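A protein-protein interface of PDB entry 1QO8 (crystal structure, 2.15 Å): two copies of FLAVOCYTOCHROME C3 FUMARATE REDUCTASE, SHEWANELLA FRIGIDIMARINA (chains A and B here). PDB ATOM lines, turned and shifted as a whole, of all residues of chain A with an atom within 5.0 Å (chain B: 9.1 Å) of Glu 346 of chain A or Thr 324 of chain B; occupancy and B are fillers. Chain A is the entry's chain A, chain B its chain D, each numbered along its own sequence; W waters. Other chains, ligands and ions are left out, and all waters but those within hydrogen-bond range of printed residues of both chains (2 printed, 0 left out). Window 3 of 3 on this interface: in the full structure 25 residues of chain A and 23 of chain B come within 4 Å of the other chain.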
ATOM      1  N   TRP A 105       6.767   5.780 -40.528  1.00  0.00           N
ATOM      2  CA  TRP A 105       6.446   6.563 -39.324  1.00  0.00           C
ATOM      3  C   TRP A 105       5.991   7.936 -39.810  1.00  0.00           C
ATOM      4  O   TRP A 105       6.576   8.524 -40.735  1.00  0.00           O
ATOM      5  CB  TRP A 105       7.655   6.533 -38.388  1.00  0.00           C
ATOM      6  CG  TRP A 105       8.507   7.762 -38.345  1.00  0.00           C
ATOM      7  CD1 TRP A 105       9.006   8.485 -39.397  1.00  0.00           C
ATOM      8  CD2 TRP A 105       8.991   8.439 -37.168  1.00  0.00           C
ATOM      9  NE1 TRP A 105       9.728   9.559 -38.956  1.00  0.00           N
ATOM     10  CE2 TRP A 105       9.734   9.565 -37.588  1.00  0.00           C
ATOM     11  CE3 TRP A 105       8.864   8.203 -35.793  1.00  0.00           C
ATOM     12  CZ2 TRP A 105      10.336  10.453 -36.697  1.00  0.00           C
ATOM     13  CZ3 TRP A 105       9.458   9.086 -34.910  1.00  0.00           C
ATOM     14  CH2 TRP A 105      10.178  10.202 -35.362  1.00  0.00           C
ATOM     15  N   VAL A 274       5.491   3.092 -32.499  1.00  0.00           N
ATOM     16  CA  VAL A 274       6.408   3.922 -33.271  1.00  0.00           C
ATOM     17  C   VAL A 274       7.231   4.930 -32.503  1.00  0.00           C
ATOM     18  O   VAL A 274       8.202   5.526 -32.956  1.00  0.00           O
ATOM     19  CB  VAL A 274       5.627   4.626 -34.366  1.00  0.00           C
ATOM     20  CG1 VAL A 274       5.134   3.737 -35.481  1.00  0.00           C
ATOM     21  CG2 VAL A 274       4.415   5.435 -33.793  1.00  0.00           C
ATOM     22  N   LYS A 275       6.953   5.172 -31.205  1.00  0.00           N
ATOM     23  CA  LYS A 275       7.704   6.070 -30.389  1.00  0.00           C
ATOM     24  C   LYS A 275       7.488   5.800 -28.920  1.00  0.00           C
ATOM     25  O   LYS A 275       6.386   5.392 -28.570  1.00  0.00           O
ATOM     26  CB  LYS A 275       7.206   7.522 -30.714  1.00  0.00           C
ATOM     27  CG  LYS A 275       8.262   8.496 -30.178  1.00  0.00           C
ATOM     28  CD  LYS A 275       7.928   9.941 -30.515  1.00  0.00           C
ATOM     29  CE  LYS A 275       9.278  10.665 -30.589  1.00  0.00           C
ATOM     30  NZ  LYS A 275       9.435  11.595 -29.432  1.00  0.00           N
ATOM     31  N   LEU A 342      15.532   0.660 -32.287  1.00  0.00           N
ATOM     32  CA  LEU A 342      15.498   2.007 -32.777  1.00  0.00           C
ATOM     33  C   LEU A 342      14.778   2.974 -31.826  1.00  0.00           C
ATOM     34  O   LEU A 342      15.325   4.047 -31.587  1.00  0.00           O
ATOM     35  CB  LEU A 342      14.830   2.118 -34.143  1.00  0.00           C
ATOM     36  CG  LEU A 342      15.596   1.287 -35.213  1.00  0.00           C
ATOM     37  CD1 LEU A 342      14.706   1.269 -36.448  1.00  0.00           C
ATOM     38  CD2 LEU A 342      17.014   1.852 -35.373  1.00  0.00           C
ATOM     39  N   MET A 343      13.616   2.655 -31.292  1.00  0.00           N
ATOM     40  CA  MET A 343      12.855   3.529 -30.407  1.00  0.00           C
ATOM     41  C   MET A 343      13.608   3.745 -29.087  1.00  0.00           C
ATOM     42  O   MET A 343      13.551   4.807 -28.468  1.00  0.00           O
ATOM     43  CB  MET A 343      11.483   2.889 -30.022  1.00  0.00           C
ATOM     44  CG  MET A 343      10.531   3.066 -31.182  1.00  0.00           C
ATOM     45  SD  MET A 343       8.891   2.380 -30.901  1.00  0.00           S
ATOM     46  CE  MET A 343       9.082   0.739 -30.309  1.00  0.00           C
ATOM     47  N   ALA A 344      14.306   2.716 -28.633  1.00  0.00           N
ATOM     48  CA  ALA A 344      15.074   2.773 -27.396  1.00  0.00           C
ATOM     49  C   ALA A 344      16.281   3.695 -27.556  1.00  0.00           C
ATOM     50  O   ALA A 344      16.543   4.609 -26.731  1.00  0.00           O
ATOM     51  CB  ALA A 344      15.442   1.450 -26.748  1.00  0.00           C
ATOM     52  N   LYS A 345      17.007   3.573 -28.623  1.00  0.00           N
ATOM     53  CA  LYS A 345      18.169   4.345 -28.963  1.00  0.00           C
ATOM     54  C   LYS A 345      17.835   5.852 -29.049  1.00  0.00           C
ATOM     55  O   LYS A 345      18.502   6.685 -28.485  1.00  0.00           O
ATOM     56  CB  LYS A 345      18.709   3.887 -30.332  1.00  0.00           C
ATOM     57  CG  LYS A 345      20.150   4.399 -30.496  1.00  0.00           C
ATOM     58  CD  LYS A 345      20.706   4.354 -31.913  1.00  0.00           C
ATOM     59  CE  LYS A 345      19.736   4.250 -33.060  1.00  0.00           C
ATOM     60  NZ  LYS A 345      20.340   4.073 -34.432  1.00  0.00           N
ATOM     61  N   GLU A 346      16.757   6.175 -29.709  1.00  0.00           N
ATOM     62  CA  GLU A 346      16.204   7.489 -29.948  1.00  0.00           C
ATOM     63  C   GLU A 346      15.907   8.219 -28.631  1.00  0.00           C
ATOM     64  O   GLU A 346      15.999   9.437 -28.663  1.00  0.00           O
ATOM     65  CB  GLU A 346      14.957   7.314 -30.801  1.00  0.00           C
ATOM     66  CG  GLU A 346      14.269   8.524 -31.351  1.00  0.00           C
ATOM     67  CD  GLU A 346      12.853   8.370 -31.826  1.00  0.00           C
ATOM     68  OE1 GLU A 346      12.354   7.277 -32.213  1.00  0.00           O
ATOM     69  OE2 GLU A 346      12.154   9.447 -31.778  1.00  0.00           O
ATOM     70  N   ILE A 347      15.552   7.608 -27.511  1.00  0.00           N
ATOM     71  CA  ILE A 347      15.370   8.307 -26.275  1.00  0.00           C
ATOM     72  C   ILE A 347      16.569   8.201 -25.357  1.00  0.00           C
ATOM     73  O   ILE A 347      16.419   8.677 -24.235  1.00  0.00           O
ATOM     74  CB  ILE A 347      14.071   7.885 -25.529  1.00  0.00           C
ATOM     75  CG1 ILE A 347      14.178   6.413 -25.196  1.00  0.00           C
ATOM     76  CG2 ILE A 347      12.874   8.195 -26.417  1.00  0.00           C
ATOM     77  CD1 ILE A 347      13.709   5.854 -23.892  1.00  0.00           C
ATOM     78  N   GLY A 348      17.706   7.632 -25.736  1.00  0.00           N
ATOM     79  CA  GLY A 348      18.902   7.612 -24.916  1.00  0.00           C
ATOM     80  C   GLY A 348      19.213   6.317 -24.216  1.00  0.00           C
ATOM     81  O   GLY A 348      20.046   6.335 -23.266  1.00  0.00           O
ATOM     82  N   LEU A 516      22.458   5.959 -20.802  1.00  0.00           N
ATOM     83  CA  LEU A 516      23.874   6.100 -21.116  1.00  0.00           C
ATOM     84  C   LEU A 516      24.817   6.112 -19.921  1.00  0.00           C
ATOM     85  O   LEU A 516      26.015   5.959 -20.135  1.00  0.00           O
ATOM     86  CB  LEU A 516      24.129   7.380 -21.928  1.00  0.00           C
ATOM     87  CG  LEU A 516      23.295   7.440 -23.223  1.00  0.00           C
ATOM     88  CD1 LEU A 516      23.689   8.717 -23.949  1.00  0.00           C
ATOM     89  CD2 LEU A 516      23.483   6.144 -24.025  1.00  0.00           C
ATOM     90  N   MET B 317      28.212   9.130 -37.939  1.00  0.00           N
ATOM     91  CA  MET B 317      28.508   8.093 -36.943  1.00  0.00           C
ATOM     92  C   MET B 317      27.847   8.379 -35.618  1.00  0.00           C
ATOM     93  O   MET B 317      27.163   7.532 -34.987  1.00  0.00           O
ATOM     94  CB  MET B 317      30.025   7.896 -36.818  1.00  0.00           C
ATOM     95  CG  MET B 317      30.551   7.261 -38.110  1.00  0.00           C
ATOM     96  SD  MET B 317      32.337   7.089 -38.058  1.00  0.00           S
ATOM     97  CE  MET B 317      32.640   5.652 -37.048  1.00  0.00           C
ATOM     98  N   ILE B 318      28.132   9.623 -35.127  1.00  0.00           N
ATOM     99  CA  ILE B 318      27.574   9.978 -33.826  1.00  0.00           C
ATOM    100  C   ILE B 318      26.056   9.947 -33.885  1.00  0.00           C
ATOM    101  O   ILE B 318      25.453   9.609 -32.855  1.00  0.00           O
ATOM    102  CB  ILE B 318      27.982  11.475 -33.543  1.00  0.00           C
ATOM    103  CG1 ILE B 318      29.490  11.508 -33.288  1.00  0.00           C
ATOM    104  CG2 ILE B 318      27.064  12.104 -32.497  1.00  0.00           C
ATOM    105  CD1 ILE B 318      29.945  10.833 -31.997  1.00  0.00           C
ATOM    106  N   ALA B 319      25.389  10.397 -34.932  1.00  0.00           N
ATOM    107  CA  ALA B 319      23.927  10.357 -34.952  1.00  0.00           C
ATOM    108  C   ALA B 319      23.399   8.893 -34.926  1.00  0.00           C
ATOM    109  O   ALA B 319      22.334   8.691 -34.360  1.00  0.00           O
ATOM    110  CB  ALA B 319      23.381  11.007 -36.199  1.00  0.00           C
ATOM    111  N   TYR B 320      24.171   7.968 -35.504  1.00  0.00           N
ATOM    112  CA  TYR B 320      23.702   6.602 -35.669  1.00  0.00           C
ATOM    113  C   TYR B 320      23.994   5.855 -34.364  1.00  0.00           C
ATOM    114  O   TYR B 320      23.090   5.138 -33.972  1.00  0.00           O
ATOM    115  CB  TYR B 320      24.276   5.883 -36.903  1.00  0.00           C
ATOM    116  CG  TYR B 320      23.366   4.699 -37.217  1.00  0.00           C
ATOM    117  CD1 TYR B 320      22.210   4.880 -37.995  1.00  0.00           C
ATOM    118  CD2 TYR B 320      23.619   3.464 -36.703  1.00  0.00           C
ATOM    119  CE1 TYR B 320      21.359   3.805 -38.261  1.00  0.00           C
ATOM    120  CE2 TYR B 320      22.797   2.369 -36.919  1.00  0.00           C
ATOM    121  CZ  TYR B 320      21.692   2.555 -37.694  1.00  0.00           C
ATOM    122  OH  TYR B 320      20.821   1.519 -37.918  1.00  0.00           O
ATOM    123  N   TYR B 321      25.114   6.195 -33.688  1.00  0.00           N
ATOM    124  CA  TYR B 321      25.443   5.504 -32.457  1.00  0.00           C
ATOM    125  C   TYR B 321      24.793   6.134 -31.268  1.00  0.00           C
ATOM    126  O   TYR B 321      24.502   5.481 -30.240  1.00  0.00           O
ATOM    127  CB  TYR B 321      26.986   5.417 -32.253  1.00  0.00           C
ATOM    128  CG  TYR B 321      27.699   4.600 -33.300  1.00  0.00           C
ATOM    129  CD1 TYR B 321      27.100   3.384 -33.751  1.00  0.00           C
ATOM    130  CD2 TYR B 321      28.898   4.898 -33.859  1.00  0.00           C
ATOM    131  CE1 TYR B 321      27.766   2.567 -34.680  1.00  0.00           C
ATOM    132  CE2 TYR B 321      29.574   4.098 -34.788  1.00  0.00           C
ATOM    133  CZ  TYR B 321      28.949   2.921 -35.197  1.00  0.00           C
ATOM    134  OH  TYR B 321      29.601   2.158 -36.160  1.00  0.00           O
ATOM    135  N   ARG B 322      24.649   7.475 -31.326  1.00  0.00           N
ATOM    136  CA  ARG B 322      24.264   8.231 -30.137  1.00  0.00           C
ATOM    137  C   ARG B 322      23.404   9.412 -30.535  1.00  0.00           C
ATOM    138  O   ARG B 322      23.813  10.576 -30.483  1.00  0.00           O
ATOM    139  CB  ARG B 322      25.499   8.725 -29.340  1.00  0.00           C
ATOM    140  CG  ARG B 322      26.215   7.615 -28.558  1.00  0.00           C
ATOM    141  CD  ARG B 322      25.471   7.270 -27.306  1.00  0.00           C
ATOM    142  NE  ARG B 322      26.083   6.316 -26.428  1.00  0.00           N
ATOM    143  CZ  ARG B 322      25.928   4.966 -26.547  1.00  0.00           C
ATOM    144  NH1 ARG B 322      25.153   4.505 -27.536  1.00  0.00           N
ATOM    145  NH2 ARG B 322      26.534   4.183 -25.664  1.00  0.00           N
ATOM    146  N   PRO B 323      22.172   9.172 -30.963  1.00  0.00           N
ATOM    147  CA  PRO B 323      21.310  10.190 -31.500  1.00  0.00           C
ATOM    148  C   PRO B 323      21.063  11.309 -30.491  1.00  0.00           C
ATOM    149  O   PRO B 323      20.797  12.408 -30.952  1.00  0.00           O
ATOM    150  CB  PRO B 323      19.973   9.508 -31.824  1.00  0.00           C
ATOM    151  CG  PRO B 323      20.100   8.158 -31.207  1.00  0.00           C
ATOM    152  CD  PRO B 323      21.532   7.835 -31.037  1.00  0.00           C
ATOM    153  N   THR B 324      21.115  11.046 -29.208  1.00  0.00           N
ATOM    154  CA  THR B 324      20.867  12.084 -28.226  1.00  0.00           C
ATOM    155  C   THR B 324      22.080  13.004 -28.120  1.00  0.00           C
ATOM    156  O   THR B 324      21.970  13.980 -27.368  1.00  0.00           O
ATOM    157  CB  THR B 324      20.511  11.604 -26.810  1.00  0.00           C
ATOM    158  OG1 THR B 324      21.637  11.027 -26.155  1.00  0.00           O
ATOM    159  CG2 THR B 324      19.330  10.649 -26.821  1.00  0.00           C
ATOM    160  N   MET B 325      23.172  12.722 -28.805  1.00  0.00           N
ATOM    161  CA  MET B 325      24.353  13.586 -28.801  1.00  0.00           C
ATOM    162  C   MET B 325      24.491  14.287 -30.138  1.00  0.00           C
ATOM    163  O   MET B 325      25.501  14.973 -30.338  1.00  0.00           O
ATOM    164  CB  MET B 325      25.652  12.788 -28.534  1.00  0.00           C
ATOM    165  CG  MET B 325      25.590  12.211 -27.084  1.00  0.00           C
ATOM    166  SD  MET B 325      27.024  11.133 -26.659  1.00  0.00           S
ATOM    167  CE  MET B 325      28.095  11.800 -27.906  1.00  0.00           C
ATOM    168  N   LYS B 326      23.536  14.149 -31.054  1.00  0.00           N
ATOM    169  CA  LYS B 326      23.780  14.610 -32.422  1.00  0.00           C
ATOM    170  C   LYS B 326      23.843  16.143 -32.632  1.00  0.00           C
ATOM    171  O   LYS B 326      24.107  16.549 -33.765  1.00  0.00           O
ATOM    172  CB  LYS B 326      22.722  14.074 -33.372  1.00  0.00           C
ATOM    173  CG  LYS B 326      21.360  14.735 -33.340  1.00  0.00           C
ATOM    174  CD  LYS B 326      20.492  13.988 -34.358  1.00  0.00           C
ATOM    175  CE  LYS B 326      19.222  14.749 -34.740  1.00  0.00           C
ATOM    176  NZ  LYS B 326      18.537  15.332 -33.556  1.00  0.00           N
ATOM    177  N   ASP B 327      23.490  16.943 -31.656  1.00  0.00           N
ATOM    178  CA  ASP B 327      23.466  18.377 -31.672  1.00  0.00           C
ATOM    179  C   ASP B 327      24.495  18.953 -30.670  1.00  0.00           C
ATOM    180  O   ASP B 327      24.411  20.132 -30.317  1.00  0.00           O
ATOM    181  CB  ASP B 327      22.099  18.932 -31.220  1.00  0.00           C
ATOM    182  CG  ASP B 327      20.994  18.662 -32.209  1.00  0.00           C
ATOM    183  OD1 ASP B 327      21.215  18.580 -33.428  1.00  0.00           O
ATOM    184  OD2 ASP B 327      19.832  18.529 -31.739  1.00  0.00           O
ATOM    185  N   MET B 328      25.424  18.099 -30.222  1.00  0.00           N
ATOM    186  CA  MET B 328      26.531  18.543 -29.424  1.00  0.00           C
ATOM    187  C   MET B 328      27.584  19.193 -30.314  1.00  0.00           C
ATOM    188  O   MET B 328      27.506  18.951 -31.514  1.00  0.00           O
ATOM    189  CB  MET B 328      27.162  17.412 -28.624  1.00  0.00           C
ATOM    190  CG  MET B 328      26.205  16.923 -27.566  1.00  0.00           C
ATOM    191  SD  MET B 328      26.997  15.733 -26.493  1.00  0.00           S
ATOM    192  CE  MET B 328      25.623  15.406 -25.377  1.00  0.00           C
ATOM    193  N   VAL B 357      30.419   6.628 -26.562  1.00  0.00           N
ATOM    194  CA  VAL B 357      30.948   7.972 -26.751  1.00  0.00           C
ATOM    195  C   VAL B 357      30.924   8.779 -25.432  1.00  0.00           C
ATOM    196  O   VAL B 357      29.925   8.853 -24.714  1.00  0.00           O
ATOM    197  CB  VAL B 357      30.197   8.836 -27.792  1.00  0.00           C
ATOM    198  CG1 VAL B 357      30.863  10.211 -28.001  1.00  0.00           C
ATOM    199  CG2 VAL B 357      30.127   8.055 -29.117  1.00  0.00           C
ATOM    200  N   ALA B 359      31.146  12.483 -23.704  1.00  0.00           N
ATOM    201  CA  ALA B 359      30.975  13.905 -23.953  1.00  0.00           C
ATOM    202  C   ALA B 359      31.376  14.725 -22.711  1.00  0.00           C
ATOM    203  O   ALA B 359      31.401  14.227 -21.588  1.00  0.00           O
ATOM    204  CB  ALA B 359      29.552  14.233 -24.325  1.00  0.00           C
ATOM    205  N   SER B 401      24.763  18.159 -19.144  1.00  0.00           N
ATOM    206  CA  SER B 401      24.496  18.052 -20.566  1.00  0.00           C
ATOM    207  C   SER B 401      23.022  17.916 -20.913  1.00  0.00           C
ATOM    208  O   SER B 401      22.554  18.639 -21.794  1.00  0.00           O
ATOM    209  CB  SER B 401      25.168  16.836 -21.215  1.00  0.00           C
ATOM    210  OG  SER B 401      26.442  16.640 -20.663  1.00  0.00           O
ATOM    211  N   ASP B 402      22.318  16.973 -20.278  1.00  0.00           N
ATOM    212  CA  ASP B 402      20.903  16.863 -20.622  1.00  0.00           C
ATOM    213  C   ASP B 402      20.249  18.214 -20.305  1.00  0.00           C
ATOM    214  O   ASP B 402      19.649  18.829 -21.193  1.00  0.00           O
ATOM    215  CB  ASP B 402      20.139  15.745 -19.904  1.00  0.00           C
ATOM    216  CG  ASP B 402      18.732  15.737 -20.489  1.00  0.00           C
ATOM    217  OD1 ASP B 402      18.648  15.474 -21.713  1.00  0.00           O
ATOM    218  OD2 ASP B 402      17.772  16.056 -19.755  1.00  0.00           O
ATOM    219  N   LEU B 405      21.190  20.721 -22.940  1.00  0.00           N
ATOM    220  CA  LEU B 405      20.589  20.443 -24.245  1.00  0.00           C
ATOM    221  C   LEU B 405      19.083  20.640 -24.224  1.00  0.00           C
ATOM    222  O   LEU B 405      18.517  20.965 -25.270  1.00  0.00           O
ATOM    223  CB  LEU B 405      20.979  19.059 -24.735  1.00  0.00           C
ATOM    224  CG  LEU B 405      22.348  18.861 -25.378  1.00  0.00           C
ATOM    225  CD1 LEU B 405      22.670  17.369 -25.459  1.00  0.00           C
ATOM    226  CD2 LEU B 405      22.400  19.465 -26.769  1.00  0.00           C
ATOM    227  N   LYS B 406      18.419  20.543 -23.079  1.00  0.00           N
ATOM    228  CA  LYS B 406      17.058  20.997 -22.894  1.00  0.00           C
ATOM    229  C   LYS B 406      16.862  22.495 -22.711  1.00  0.00           C
ATOM    230  O   LYS B 406      15.824  22.829 -22.102  1.00  0.00           O
ATOM    231  CB  LYS B 406      16.440  20.366 -21.625  1.00  0.00           C
ATOM    232  CG  LYS B 406      15.867  18.979 -21.806  1.00  0.00           C
ATOM    233  CD  LYS B 406      15.812  18.215 -20.486  1.00  0.00           C
ATOM    234  CE  LYS B 406      14.393  18.169 -19.940  1.00  0.00           C
ATOM    235  NZ  LYS B 406      14.094  16.904 -19.211  1.00  0.00           N
ATOM    236  N   GLN B 410      20.084  25.256 -26.988  1.00  0.00           N
ATOM    237  CA  GLN B 410      20.906  24.193 -26.451  1.00  0.00           C
ATOM    238  C   GLN B 410      22.311  24.648 -26.086  1.00  0.00           C
ATOM    239  O   GLN B 410      23.305  24.022 -26.440  1.00  0.00           O
ATOM    240  CB  GLN B 410      20.884  22.987 -27.412  1.00  0.00           C
ATOM    241  CG  GLN B 410      19.446  22.571 -27.716  1.00  0.00           C
ATOM    242  CD  GLN B 410      19.346  21.213 -28.362  1.00  0.00           C
ATOM    243  OE1 GLN B 410      19.524  21.076 -29.577  1.00  0.00           O
ATOM    244  NE2 GLN B 410      19.062  20.214 -27.543  1.00  0.00           N
ATOM    245  N   PRO B 496      27.399  21.145 -24.169  1.00  0.00           N
ATOM    246  CA  PRO B 496      27.945  19.791 -24.097  1.00  0.00           C
ATOM    247  C   PRO B 496      28.609  19.432 -25.418  1.00  0.00           C
ATOM    248  O   PRO B 496      28.086  19.724 -26.473  1.00  0.00           O
ATOM    249  CB  PRO B 496      26.738  18.921 -23.774  1.00  0.00           C
ATOM    250  CG  PRO B 496      25.606  19.683 -24.388  1.00  0.00           C
ATOM    251  CD  PRO B 496      25.913  21.140 -24.092  1.00  0.00           C
ATOM    252  N   ILE B 498      31.101  16.513 -27.713  1.00  0.00           N
ATOM    253  CA  ILE B 498      31.742  15.212 -27.925  1.00  0.00           C
ATOM    254  C   ILE B 498      33.242  15.306 -27.693  1.00  0.00           C
ATOM    255  O   ILE B 498      33.927  16.116 -28.334  1.00  0.00           O
ATOM    256  CB  ILE B 498      31.462  14.638 -29.355  1.00  0.00           C
ATOM    257  CG1 ILE B 498      29.932  14.495 -29.618  1.00  0.00           C
ATOM    258  CG2 ILE B 498      32.025  13.238 -29.466  1.00  0.00           C
ATOM    259  CD1 ILE B 498      29.704  14.661 -31.098  1.00  0.00           C
HETATM  260  O   HOH W   1      20.401   1.152 -34.881  1.00  0.00           O
HETATM  261  O   HOH W   2      20.012   7.485 -35.027  1.00  0.00           O
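Of the printed residues of chain A, Pro 323 of chain B touches Lys 345 (3.5 Å).
Of the printed residues of chain B, Ile 347 of chain A touches Thr 324 (3.97 Å).
Printed residues of chain B within 4 Å of Lys 345 of chain A: Tyr 320 and Pro 323.
Of the printed residues of chain B, Leu 516 of chain A touches Arg 322 and Thr 324.
Met 325 of chain B touches none of the printed residues of chain A.
Tyr 321 of chain B touches none of the printed residues of chain A.
The nearest printed residue of chain B that does not touch Lys 345 of chain A is Tyr 321 of chain B (4.3 Å).
No position is printed for both chains.
Of the 7 pairs that touch across the chains among the printed residues, none has its exchanged pair printed and touching as well.
The backbone NH (N) of Leu 516 of chain A lies close to the backbone carbonyl oxygen (O) of Gly 348 of chain A, 3.5 Å away.
Pro 323 of chain B touches Lys 345 of chain A (CG to O, 3.5 Å).
CG2 of Thr 324 of chain B touches O of Glu 346 of chain A, at 3.99 Å.
Thr 324 of chain B touches Ile 347 of chain A.
Thr 324 of chain B touches Gly 348 of chain A.
Leu 516 of chain A touches Arg 322 of chain B.
Leu 516 of chain A touches Thr 324 of chain B.
Water W2 lies within hydrogen-bond range of O of Ala 319 of chain B (2.7 Å) and NZ of Lys 345 of chain A (3.5 Å).
Water W1 bridges NZ of Lys 345 of chain A (3.0 Å) and OH of Tyr 320 of chain B (3.1 Å).
Printed residues of chain A that touch a printed residue of chain B: Lys 345, Glu 346, Ile 347, Gly 348 and Leu 516.
Hydrophobic or aromatic side chains of chain A that line the printed part of chain B: Leu 516.
Along chain A the printed residues that touch a printed residue of chain B span positions 345 to 516.
Of the 21 printed residues of chain B, 4 touch a printed residue of chain A.
Printed residues of chain B that touch a printed residue of chain A: Tyr 320, Arg 322, Pro 323 and Thr 324.
Hydrophobic or aromatic side chains of chain B that line the printed part of chain A: Tyr 320 and Pro 323.
Along chain B the printed residues that touch a printed residue of chain A span positions 320 to 324.
Among the printed residues, 7 pairs touch across the chains.
Among the printed residues, no Asp or Glu carboxylate lies within 4 Å of a Lys or Arg side-chain nitrogen of the other chain.
O of Tyr 320 of chain B sits at hydrogen-bond distance from NZ of Lys 345 of chain A (3.0 Å).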
